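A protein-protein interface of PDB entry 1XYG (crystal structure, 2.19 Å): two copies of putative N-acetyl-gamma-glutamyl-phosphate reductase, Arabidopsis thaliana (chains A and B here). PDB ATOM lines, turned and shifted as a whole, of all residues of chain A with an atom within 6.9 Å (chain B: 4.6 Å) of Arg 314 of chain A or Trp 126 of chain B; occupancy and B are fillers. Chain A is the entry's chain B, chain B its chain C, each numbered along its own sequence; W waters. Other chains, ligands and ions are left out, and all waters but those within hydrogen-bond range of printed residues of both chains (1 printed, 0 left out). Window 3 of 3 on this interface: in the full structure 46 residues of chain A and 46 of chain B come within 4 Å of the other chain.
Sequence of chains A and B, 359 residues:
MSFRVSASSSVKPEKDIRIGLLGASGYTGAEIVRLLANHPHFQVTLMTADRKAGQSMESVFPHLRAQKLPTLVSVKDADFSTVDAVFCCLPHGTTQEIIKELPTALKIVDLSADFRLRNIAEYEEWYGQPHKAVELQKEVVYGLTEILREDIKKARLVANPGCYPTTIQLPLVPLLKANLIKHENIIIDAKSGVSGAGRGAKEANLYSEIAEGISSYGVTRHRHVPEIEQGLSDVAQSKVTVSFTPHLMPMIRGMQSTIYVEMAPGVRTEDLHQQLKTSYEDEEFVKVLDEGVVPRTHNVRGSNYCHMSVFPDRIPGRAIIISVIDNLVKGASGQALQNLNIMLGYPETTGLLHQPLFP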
ATOM      1  N   PRO A 312      27.870  -2.894  31.363  1.00  0.00           N
ATOM      2  CA  PRO A 312      27.470  -1.505  31.558  1.00  0.00           C
ATOM      3  C   PRO A 312      26.527  -1.135  30.414  1.00  0.00           C
ATOM      4  O   PRO A 312      26.646  -1.658  29.302  1.00  0.00           O
ATOM      5  CB  PRO A 312      28.799  -0.754  31.486  1.00  0.00           C
ATOM      6  CG  PRO A 312      29.615  -1.603  30.570  1.00  0.00           C
ATOM      7  CD  PRO A 312      29.307  -2.987  31.054  1.00  0.00           C
ATOM      8  N   ASP A 313      25.564  -0.271  30.696  1.00  0.00           N
ATOM      9  CA  ASP A 313      24.642   0.177  29.674  1.00  0.00           C
ATOM     10  C   ASP A 313      25.285   1.441  29.104  1.00  0.00           C
ATOM     11  O   ASP A 313      26.052   2.117  29.800  1.00  0.00           O
ATOM     12  CB  ASP A 313      23.276   0.495  30.296  1.00  0.00           C
ATOM     13  CG  ASP A 313      22.221   0.806  29.252  1.00  0.00           C
ATOM     14  OD1 ASP A 313      22.306   1.884  28.628  1.00  0.00           O
ATOM     15  OD2 ASP A 313      21.314  -0.037  29.053  1.00  0.00           O
ATOM     16  N   ARG A 314      25.001   1.756  27.846  1.00  0.00           N
ATOM     17  CA  ARG A 314      25.569   2.953  27.241  1.00  0.00           C
ATOM     18  C   ARG A 314      25.031   4.171  27.991  1.00  0.00           C
ATOM     19  O   ARG A 314      25.716   5.190  28.120  1.00  0.00           O
ATOM     20  CB  ARG A 314      25.193   3.033  25.757  1.00  0.00           C
ATOM     21  CG  ARG A 314      25.775   4.236  25.035  1.00  0.00           C
ATOM     22  CD  ARG A 314      25.467   4.188  23.549  1.00  0.00           C
ATOM     23  NE  ARG A 314      25.796   5.440  22.881  1.00  0.00           N
ATOM     24  CZ  ARG A 314      27.018   5.963  22.806  1.00  0.00           C
ATOM     25  NH1 ARG A 314      28.051   5.341  23.364  1.00  0.00           N
ATOM     26  NH2 ARG A 314      27.211   7.113  22.176  1.00  0.00           N
ATOM     27  N   ILE A 315      23.799   4.054  28.477  1.00  0.00           N
ATOM     28  CA  ILE A 315      23.160   5.128  29.225  1.00  0.00           C
ATOM     29  C   ILE A 315      23.782   5.152  30.621  1.00  0.00           C
ATOM     30  O   ILE A 315      23.680   4.186  31.374  1.00  0.00           O
ATOM     31  CB  ILE A 315      21.639   4.894  29.351  1.00  0.00           C
ATOM     32  CG1 ILE A 315      20.977   5.001  27.972  1.00  0.00           C
ATOM     33  CG2 ILE A 315      21.037   5.888  30.334  1.00  0.00           C
ATOM     34  CD1 ILE A 315      19.483   4.660  27.982  1.00  0.00           C
ATOM     35  N   PRO A 316      24.439   6.260  30.983  1.00  0.00           N
ATOM     36  CA  PRO A 316      25.072   6.367  32.302  1.00  0.00           C
ATOM     37  C   PRO A 316      24.130   6.049  33.466  1.00  0.00           C
ATOM     38  O   PRO A 316      22.984   6.500  33.505  1.00  0.00           O
ATOM     39  CB  PRO A 316      25.573   7.809  32.328  1.00  0.00           C
ATOM     40  CG  PRO A 316      25.825   8.107  30.857  1.00  0.00           C
ATOM     41  CD  PRO A 316      24.621   7.494  30.198  1.00  0.00           C
ATOM     42  N   GLY A 317      24.633   5.255  34.405  1.00  0.00           N
ATOM     43  CA  GLY A 317      23.846   4.887  35.563  1.00  0.00           C
ATOM     44  C   GLY A 317      23.093   3.587  35.393  1.00  0.00           C
ATOM     45  O   GLY A 317      22.576   3.031  36.361  1.00  0.00           O
ATOM     46  N   ARG A 318      23.030   3.095  34.162  1.00  0.00           N
ATOM     47  CA  ARG A 318      22.324   1.858  33.889  1.00  0.00           C
ATOM     48  C   ARG A 318      23.255   0.681  33.642  1.00  0.00           C
ATOM     49  O   ARG A 318      24.416   0.858  33.272  1.00  0.00           O
ATOM     50  CB  ARG A 318      21.383   2.043  32.695  1.00  0.00           C
ATOM     51  CG  ARG A 318      19.969   2.364  33.103  1.00  0.00           C
ATOM     52  CD  ARG A 318      19.067   2.592  31.906  1.00  0.00           C
ATOM     53  NE  ARG A 318      17.685   2.734  32.340  1.00  0.00           N
ATOM     54  CZ  ARG A 318      16.934   1.722  32.760  1.00  0.00           C
ATOM     55  NH1 ARG A 318      17.437   0.494  32.792  1.00  0.00           N
ATOM     56  NH2 ARG A 318      15.690   1.944  33.161  1.00  0.00           N
ATOM     57  N   ALA A 319      22.732  -0.520  33.864  1.00  0.00           N
ATOM     58  CA  ALA A 319      23.493  -1.742  33.668  1.00  0.00           C
ATOM     59  C   ALA A 319      22.625  -2.767  32.947  1.00  0.00           C
ATOM     60  O   ALA A 319      21.392  -2.663  32.940  1.00  0.00           O
ATOM     61  CB  ALA A 319      23.960  -2.301  35.016  1.00  0.00           C
ATOM     62  N   ILE A 320      23.274  -3.756  32.341  1.00  0.00           N
ATOM     63  CA  ILE A 320      22.565  -4.799  31.622  1.00  0.00           C
ATOM     64  C   ILE A 320      22.939  -6.156  32.179  1.00  0.00           C
ATOM     65  O   ILE A 320      24.122  -6.475  32.319  1.00  0.00           O
ATOM     66  CB  ILE A 320      22.908  -4.781  30.121  1.00  0.00           C
ATOM     67  CG1 ILE A 320      22.519  -3.432  29.517  1.00  0.00           C
ATOM     68  CG2 ILE A 320      22.212  -5.931  29.420  1.00  0.00           C
ATOM     69  CD1 ILE A 320      22.862  -3.289  28.058  1.00  0.00           C
ATOM     70  N   GLU B 122      33.569  11.090  14.572  1.00  0.00           N
ATOM     71  CA  GLU B 122      32.665  10.049  15.023  1.00  0.00           C
ATOM     72  C   GLU B 122      32.922   8.766  14.235  1.00  0.00           C
ATOM     73  O   GLU B 122      32.956   7.679  14.808  1.00  0.00           O
ATOM     74  CB  GLU B 122      31.235  10.546  14.831  1.00  0.00           C
ATOM     75  CG  GLU B 122      30.181   9.880  15.665  1.00  0.00           C
ATOM     76  CD  GLU B 122      29.019  10.814  15.920  1.00  0.00           C
ATOM     77  OE1 GLU B 122      29.069  11.565  16.917  1.00  0.00           O
ATOM     78  OE2 GLU B 122      28.065  10.819  15.115  1.00  0.00           O
ATOM     79  N   TYR B 123      33.110   8.895  12.923  1.00  0.00           N
ATOM     80  CA  TYR B 123      33.376   7.735  12.076  1.00  0.00           C
ATOM     81  C   TYR B 123      34.674   7.068  12.502  1.00  0.00           C
ATOM     82  O   TYR B 123      34.768   5.844  12.575  1.00  0.00           O
ATOM     83  CB  TYR B 123      33.496   8.146  10.604  1.00  0.00           C
ATOM     84  CG  TYR B 123      33.990   7.019   9.713  1.00  0.00           C
ATOM     85  CD1 TYR B 123      33.140   5.980   9.332  1.00  0.00           C
ATOM     86  CD2 TYR B 123      35.320   6.965   9.293  1.00  0.00           C
ATOM     87  CE1 TYR B 123      33.603   4.906   8.554  1.00  0.00           C
ATOM     88  CE2 TYR B 123      35.793   5.899   8.519  1.00  0.00           C
ATOM     89  CZ  TYR B 123      34.927   4.870   8.154  1.00  0.00           C
ATOM     90  OH  TYR B 123      35.388   3.792   7.420  1.00  0.00           O
ATOM     91  N   GLU B 124      35.677   7.890  12.771  1.00  0.00           N
ATOM     92  CA  GLU B 124      36.983   7.394  13.172  1.00  0.00           C
ATOM     93  C   GLU B 124      37.008   6.653  14.503  1.00  0.00           C
ATOM     94  O   GLU B 124      37.631   5.591  14.623  1.00  0.00           O
ATOM     95  CB  GLU B 124      37.971   8.552  13.178  1.00  0.00           C
ATOM     96  CG  GLU B 124      38.259   9.000  11.762  1.00  0.00           C
ATOM     97  CD  GLU B 124      39.203  10.172  11.669  1.00  0.00           C
ATOM     98  OE1 GLU B 124      40.163  10.228  12.458  1.00  0.00           O
ATOM     99  OE2 GLU B 124      39.001  11.034  10.791  1.00  0.00           O
ATOM    100  N   GLU B 125      36.324   7.195  15.504  1.00  0.00           N
ATOM    101  CA  GLU B 125      36.307   6.545  16.808  1.00  0.00           C
ATOM    102  C   GLU B 125      35.550   5.221  16.771  1.00  0.00           C
ATOM    103  O   GLU B 125      35.937   4.262  17.438  1.00  0.00           O
ATOM    104  CB  GLU B 125      35.691   7.457  17.869  1.00  0.00           C
ATOM    105  CG  GLU B 125      34.194   7.627  17.763  1.00  0.00           C
ATOM    106  CD  GLU B 125      33.574   8.113  19.059  1.00  0.00           C
ATOM    107  OE1 GLU B 125      33.690   7.393  20.070  1.00  0.00           O
ATOM    108  OE2 GLU B 125      32.971   9.206  19.074  1.00  0.00           O
ATOM    109  N   TRP B 126      34.481   5.156  15.987  1.00  0.00           N
ATOM    110  CA  TRP B 126      33.702   3.930  15.910  1.00  0.00           C
ATOM    111  C   TRP B 126      34.179   2.909  14.891  1.00  0.00           C
ATOM    112  O   TRP B 126      33.881   1.724  15.022  1.00  0.00           O
ATOM    113  CB  TRP B 126      32.233   4.239  15.633  1.00  0.00           C
ATOM    114  CG  TRP B 126      31.516   4.797  16.802  1.00  0.00           C
ATOM    115  CD1 TRP B 126      31.359   6.112  17.115  1.00  0.00           C
ATOM    116  CD2 TRP B 126      30.867   4.062  17.833  1.00  0.00           C
ATOM    117  NE1 TRP B 126      30.649   6.248  18.279  1.00  0.00           N
ATOM    118  CE2 TRP B 126      30.328   4.988  18.749  1.00  0.00           C
ATOM    119  CE3 TRP B 126      30.677   2.690  18.082  1.00  0.00           C
ATOM    120  CZ2 TRP B 126      29.620   4.615  19.888  1.00  0.00           C
ATOM    121  CZ3 TRP B 126      29.971   2.308  19.216  1.00  0.00           C
ATOM    122  CH2 TRP B 126      29.449   3.268  20.103  1.00  0.00           C
ATOM    123  N   TYR B 127      34.916   3.347  13.875  1.00  0.00           N
ATOM    124  CA  TYR B 127      35.373   2.415  12.851  1.00  0.00           C
ATOM    125  C   TYR B 127      36.866   2.131  12.831  1.00  0.00           C
ATOM    126  O   TYR B 127      37.345   1.349  12.010  1.00  0.00           O
ATOM    127  CB  TYR B 127      34.859   2.878  11.487  1.00  0.00           C
ATOM    128  CG  TYR B 127      33.395   2.538  11.313  1.00  0.00           C
ATOM    129  CD1 TYR B 127      33.010   1.269  10.881  1.00  0.00           C
ATOM    130  CD2 TYR B 127      32.395   3.437  11.683  1.00  0.00           C
ATOM    131  CE1 TYR B 127      31.670   0.896  10.824  1.00  0.00           C
ATOM    132  CE2 TYR B 127      31.039   3.069  11.636  1.00  0.00           C
ATOM    133  CZ  TYR B 127      30.689   1.796  11.207  1.00  0.00           C
ATOM    134  OH  TYR B 127      29.366   1.407  11.180  1.00  0.00           O
ATOM    135  N   GLY B 128      37.594   2.753  13.751  1.00  0.00           N
ATOM    136  CA  GLY B 128      39.024   2.518  13.864  1.00  0.00           C
ATOM    137  C   GLY B 128      39.976   2.971  12.766  1.00  0.00           C
ATOM    138  O   GLY B 128      41.074   2.420  12.644  1.00  0.00           O
ATOM    139  N   THR B 220      26.674  -2.926  24.856  1.00  0.00           N
ATOM    140  CA  THR B 220      27.218  -1.614  25.207  1.00  0.00           C
ATOM    141  C   THR B 220      27.648  -0.793  23.994  1.00  0.00           C
ATOM    142  O   THR B 220      27.206   0.339  23.818  1.00  0.00           O
ATOM    143  CB  THR B 220      28.437  -1.726  26.155  1.00  0.00           C
ATOM    144  OG1 THR B 220      28.094  -2.525  27.295  1.00  0.00           O
ATOM    145  CG2 THR B 220      28.859  -0.338  26.633  1.00  0.00           C
ATOM    146  N   ARG B 221      28.525  -1.360  23.172  1.00  0.00           N
ATOM    147  CA  ARG B 221      29.014  -0.665  21.988  1.00  0.00           C
ATOM    148  C   ARG B 221      28.885  -1.518  20.742  1.00  0.00           C
ATOM    149  O   ARG B 221      29.460  -2.599  20.649  1.00  0.00           O
ATOM    150  CB  ARG B 221      30.484  -0.256  22.165  1.00  0.00           C
ATOM    151  CG  ARG B 221      30.699   0.891  23.143  1.00  0.00           C
ATOM    152  CD  ARG B 221      32.174   1.077  23.535  1.00  0.00           C
ATOM    153  NE  ARG B 221      32.998   1.753  22.524  1.00  0.00           N
ATOM    154  CZ  ARG B 221      32.893   3.039  22.186  1.00  0.00           C
ATOM    155  NH1 ARG B 221      33.695   3.549  21.259  1.00  0.00           N
ATOM    156  NH2 ARG B 221      31.988   3.814  22.770  1.00  0.00           N
ATOM    157  N   HIS B 222      28.107  -1.029  19.792  1.00  0.00           N
ATOM    158  CA  HIS B 222      27.919  -1.710  18.517  1.00  0.00           C
ATOM    159  C   HIS B 222      27.940  -0.592  17.488  1.00  0.00           C
ATOM    160  O   HIS B 222      27.377   0.475  17.722  1.00  0.00           O
ATOM    161  CB  HIS B 222      26.586  -2.458  18.478  1.00  0.00           C
ATOM    162  CG  HIS B 222      26.346  -3.177  17.189  1.00  0.00           C
ATOM    163  ND1 HIS B 222      25.845  -2.548  16.068  1.00  0.00           N
ATOM    164  CD2 HIS B 222      26.591  -4.458  16.824  1.00  0.00           C
ATOM    165  CE1 HIS B 222      25.794  -3.411  15.070  1.00  0.00           C
ATOM    166  NE2 HIS B 222      26.240  -4.578  15.501  1.00  0.00           N
ATOM    167  N   ARG B 223      28.595  -0.830  16.358  1.00  0.00           N
ATOM    168  CA  ARG B 223      28.724   0.197  15.326  1.00  0.00           C
ATOM    169  C   ARG B 223      27.456   0.892  14.844  1.00  0.00           C
ATOM    170  O   ARG B 223      27.530   1.975  14.261  1.00  0.00           O
ATOM    171  CB  ARG B 223      29.508  -0.366  14.143  1.00  0.00           C
ATOM    172  CG  ARG B 223      30.978  -0.537  14.478  1.00  0.00           C
ATOM    173  CD  ARG B 223      31.758  -1.239  13.396  1.00  0.00           C
ATOM    174  NE  ARG B 223      33.183  -1.238  13.709  1.00  0.00           N
ATOM    175  CZ  ARG B 223      34.112  -1.858  12.988  1.00  0.00           C
ATOM    176  NH1 ARG B 223      35.387  -1.796  13.357  1.00  0.00           N
ATOM    177  NH2 ARG B 223      33.768  -2.540  11.904  1.00  0.00           N
ATOM    178  N   VAL B 225      25.186   2.016  16.837  1.00  0.00           N
ATOM    179  CA  VAL B 225      24.828   3.009  17.849  1.00  0.00           C
ATOM    180  C   VAL B 225      24.919   4.444  17.327  1.00  0.00           C
ATOM    181  O   VAL B 225      23.918   5.163  17.329  1.00  0.00           O
ATOM    182  CB  VAL B 225      25.699   2.856  19.131  1.00  0.00           C
ATOM    183  CG1 VAL B 225      25.478   4.028  20.068  1.00  0.00           C
ATOM    184  CG2 VAL B 225      25.351   1.552  19.843  1.00  0.00           C
ATOM    185  N   PRO B 226      26.109   4.878  16.858  1.00  0.00           N
ATOM    186  CA  PRO B 226      26.230   6.253  16.350  1.00  0.00           C
ATOM    187  C   PRO B 226      25.282   6.568  15.197  1.00  0.00           C
ATOM    188  O   PRO B 226      24.794   7.697  15.079  1.00  0.00           O
ATOM    189  CB  PRO B 226      27.707   6.357  15.957  1.00  0.00           C
ATOM    190  CG  PRO B 226      28.090   4.937  15.642  1.00  0.00           C
ATOM    191  CD  PRO B 226      27.387   4.154  16.717  1.00  0.00           C
ATOM    192  N   GLU B 229      21.793   7.062  16.867  1.00  0.00           N
ATOM    193  CA  GLU B 229      21.748   8.332  17.585  1.00  0.00           C
ATOM    194  C   GLU B 229      21.789   9.544  16.650  1.00  0.00           C
ATOM    195  O   GLU B 229      21.152  10.564  16.923  1.00  0.00           O
ATOM    196  CB  GLU B 229      22.886   8.394  18.614  1.00  0.00           C
ATOM    197  CG  GLU B 229      22.923   7.186  19.559  1.00  0.00           C
ATOM    198  CD  GLU B 229      23.864   7.349  20.752  1.00  0.00           C
ATOM    199  OE1 GLU B 229      24.901   8.030  20.614  1.00  0.00           O
ATOM    200  OE2 GLU B 229      23.568   6.776  21.829  1.00  0.00           O
ATOM    201  N   THR B 241      21.068   9.812  23.516  1.00  0.00           N
ATOM    202  CA  THR B 241      21.884   8.669  23.904  1.00  0.00           C
ATOM    203  C   THR B 241      20.943   7.506  24.181  1.00  0.00           C
ATOM    204  O   THR B 241      20.103   7.579  25.075  1.00  0.00           O
ATOM    205  CB  THR B 241      22.716   8.949  25.175  1.00  0.00           C
ATOM    206  OG1 THR B 241      23.690   9.964  24.896  1.00  0.00           O
ATOM    207  CG2 THR B 241      23.445   7.682  25.617  1.00  0.00           C
ATOM    208  N   VAL B 242      21.085   6.435  23.409  1.00  0.00           N
ATOM    209  CA  VAL B 242      20.228   5.271  23.575  1.00  0.00           C
ATOM    210  C   VAL B 242      20.983   4.058  24.106  1.00  0.00           C
ATOM    211  O   VAL B 242      22.212   4.060  24.224  1.00  0.00           O
ATOM    212  CB  VAL B 242      19.574   4.860  22.225  1.00  0.00           C
ATOM    213  CG1 VAL B 242      18.985   6.086  21.536  1.00  0.00           C
ATOM    214  CG2 VAL B 242      20.607   4.184  21.321  1.00  0.00           C
HETATM  215  O   HOH W   1      28.447   2.897  24.409  1.00  0.00           O
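The side-chain hydroxyl (OG1) of Thr 220 of chain B sits at hydrogen-bond distance from the backbone carbonyl oxygen (O) of Pro 312 of chain A (2.6 Å).
The guanidinium group (NE) of Arg 314 of chain A lies within salt-bridge range of the side-chain carboxylate (OE2) of Glu 229 of chain B, at 2.8 Å.
OD1 of Asp 313 of chain A sits at hydrogen-bond distance from N of Ile 315 of chain A, at 2.6 Å.
The backbone carbonyl oxygen (O) of Trp 126 of chain B is in hydrogen-bond range of the guanidinium group (NE) of Arg 223 of chain B.
OE2 of Glu 229 of chain B sits at hydrogen-bond distance from N of Val 242 of chain B (3.0 Å).
Trp 126 of chain B touches Arg 314 of chain A.
O of Thr 220 of chain B touches CB of Arg 314 of chain A, at 3.9 Å.
Arg 314 of chain A touches Val 225 of chain B.
CD of Arg 314 of chain A touches O of Val 242 of chain B, at 3.3 Å.
CG1 of Ile 315 of chain A touches O of Thr 241 of chain B, at 3.98 Å.
CG1 of Ile 315 of chain A touches C of Val 242 of chain B, 3.98 Å away.
Printed residues of chain B within 4 Å of Arg 314 of chain A: Trp 126 (3.9 Å), Thr 220 (3.9 Å), Val 225 (3.2 Å), Glu 229 (2.8 Å) and Val 242 (3.3 Å).
Of chain A, only Arg 314 (3.9 Å) comes within 4 Å of Trp 126 of chain B.
Of the printed residues of chain A, Thr 220 of chain B touches Pro 312 (2.6 Å) and Arg 314 (3.9 Å).
Printed residues of chain A within 4 Å of Val 225 of chain B: Arg 314 (3.2 Å).
Asp 313 of chain A touches none of the printed residues of chain B.
The nearest printed residue of chain A that does not touch Trp 126 of chain B is Asp 313 of chain A (10.1 Å).
Of the 9 printed residues of chain A, 3 touch a printed residue of chain B.
Printed residues of chain A that touch a printed residue of chain B: Pro 312, Arg 314 and Ile 315.
Along chain A the printed residues that touch a printed residue of chain B span positions 312 to 315.
Among the printed residues, 8 pairs touch across the chains.
Among the printed residues, Asp or Glu carboxylates within 4 Å of a Lys or Arg side-chain nitrogen of the other chain: Arg 314 of chain A with Glu 229 of chain B (2.8 Å).
No position is printed for both chains.
Of the 8 pairs that touch across the chains among the printed residues, none has its exchanged pair printed and touching as well.
Water W1 lies within hydrogen-bond range of NH1 of Arg 314 of chain A (2.7 Å) and O of Thr 220 of chain B (2.9 Å).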
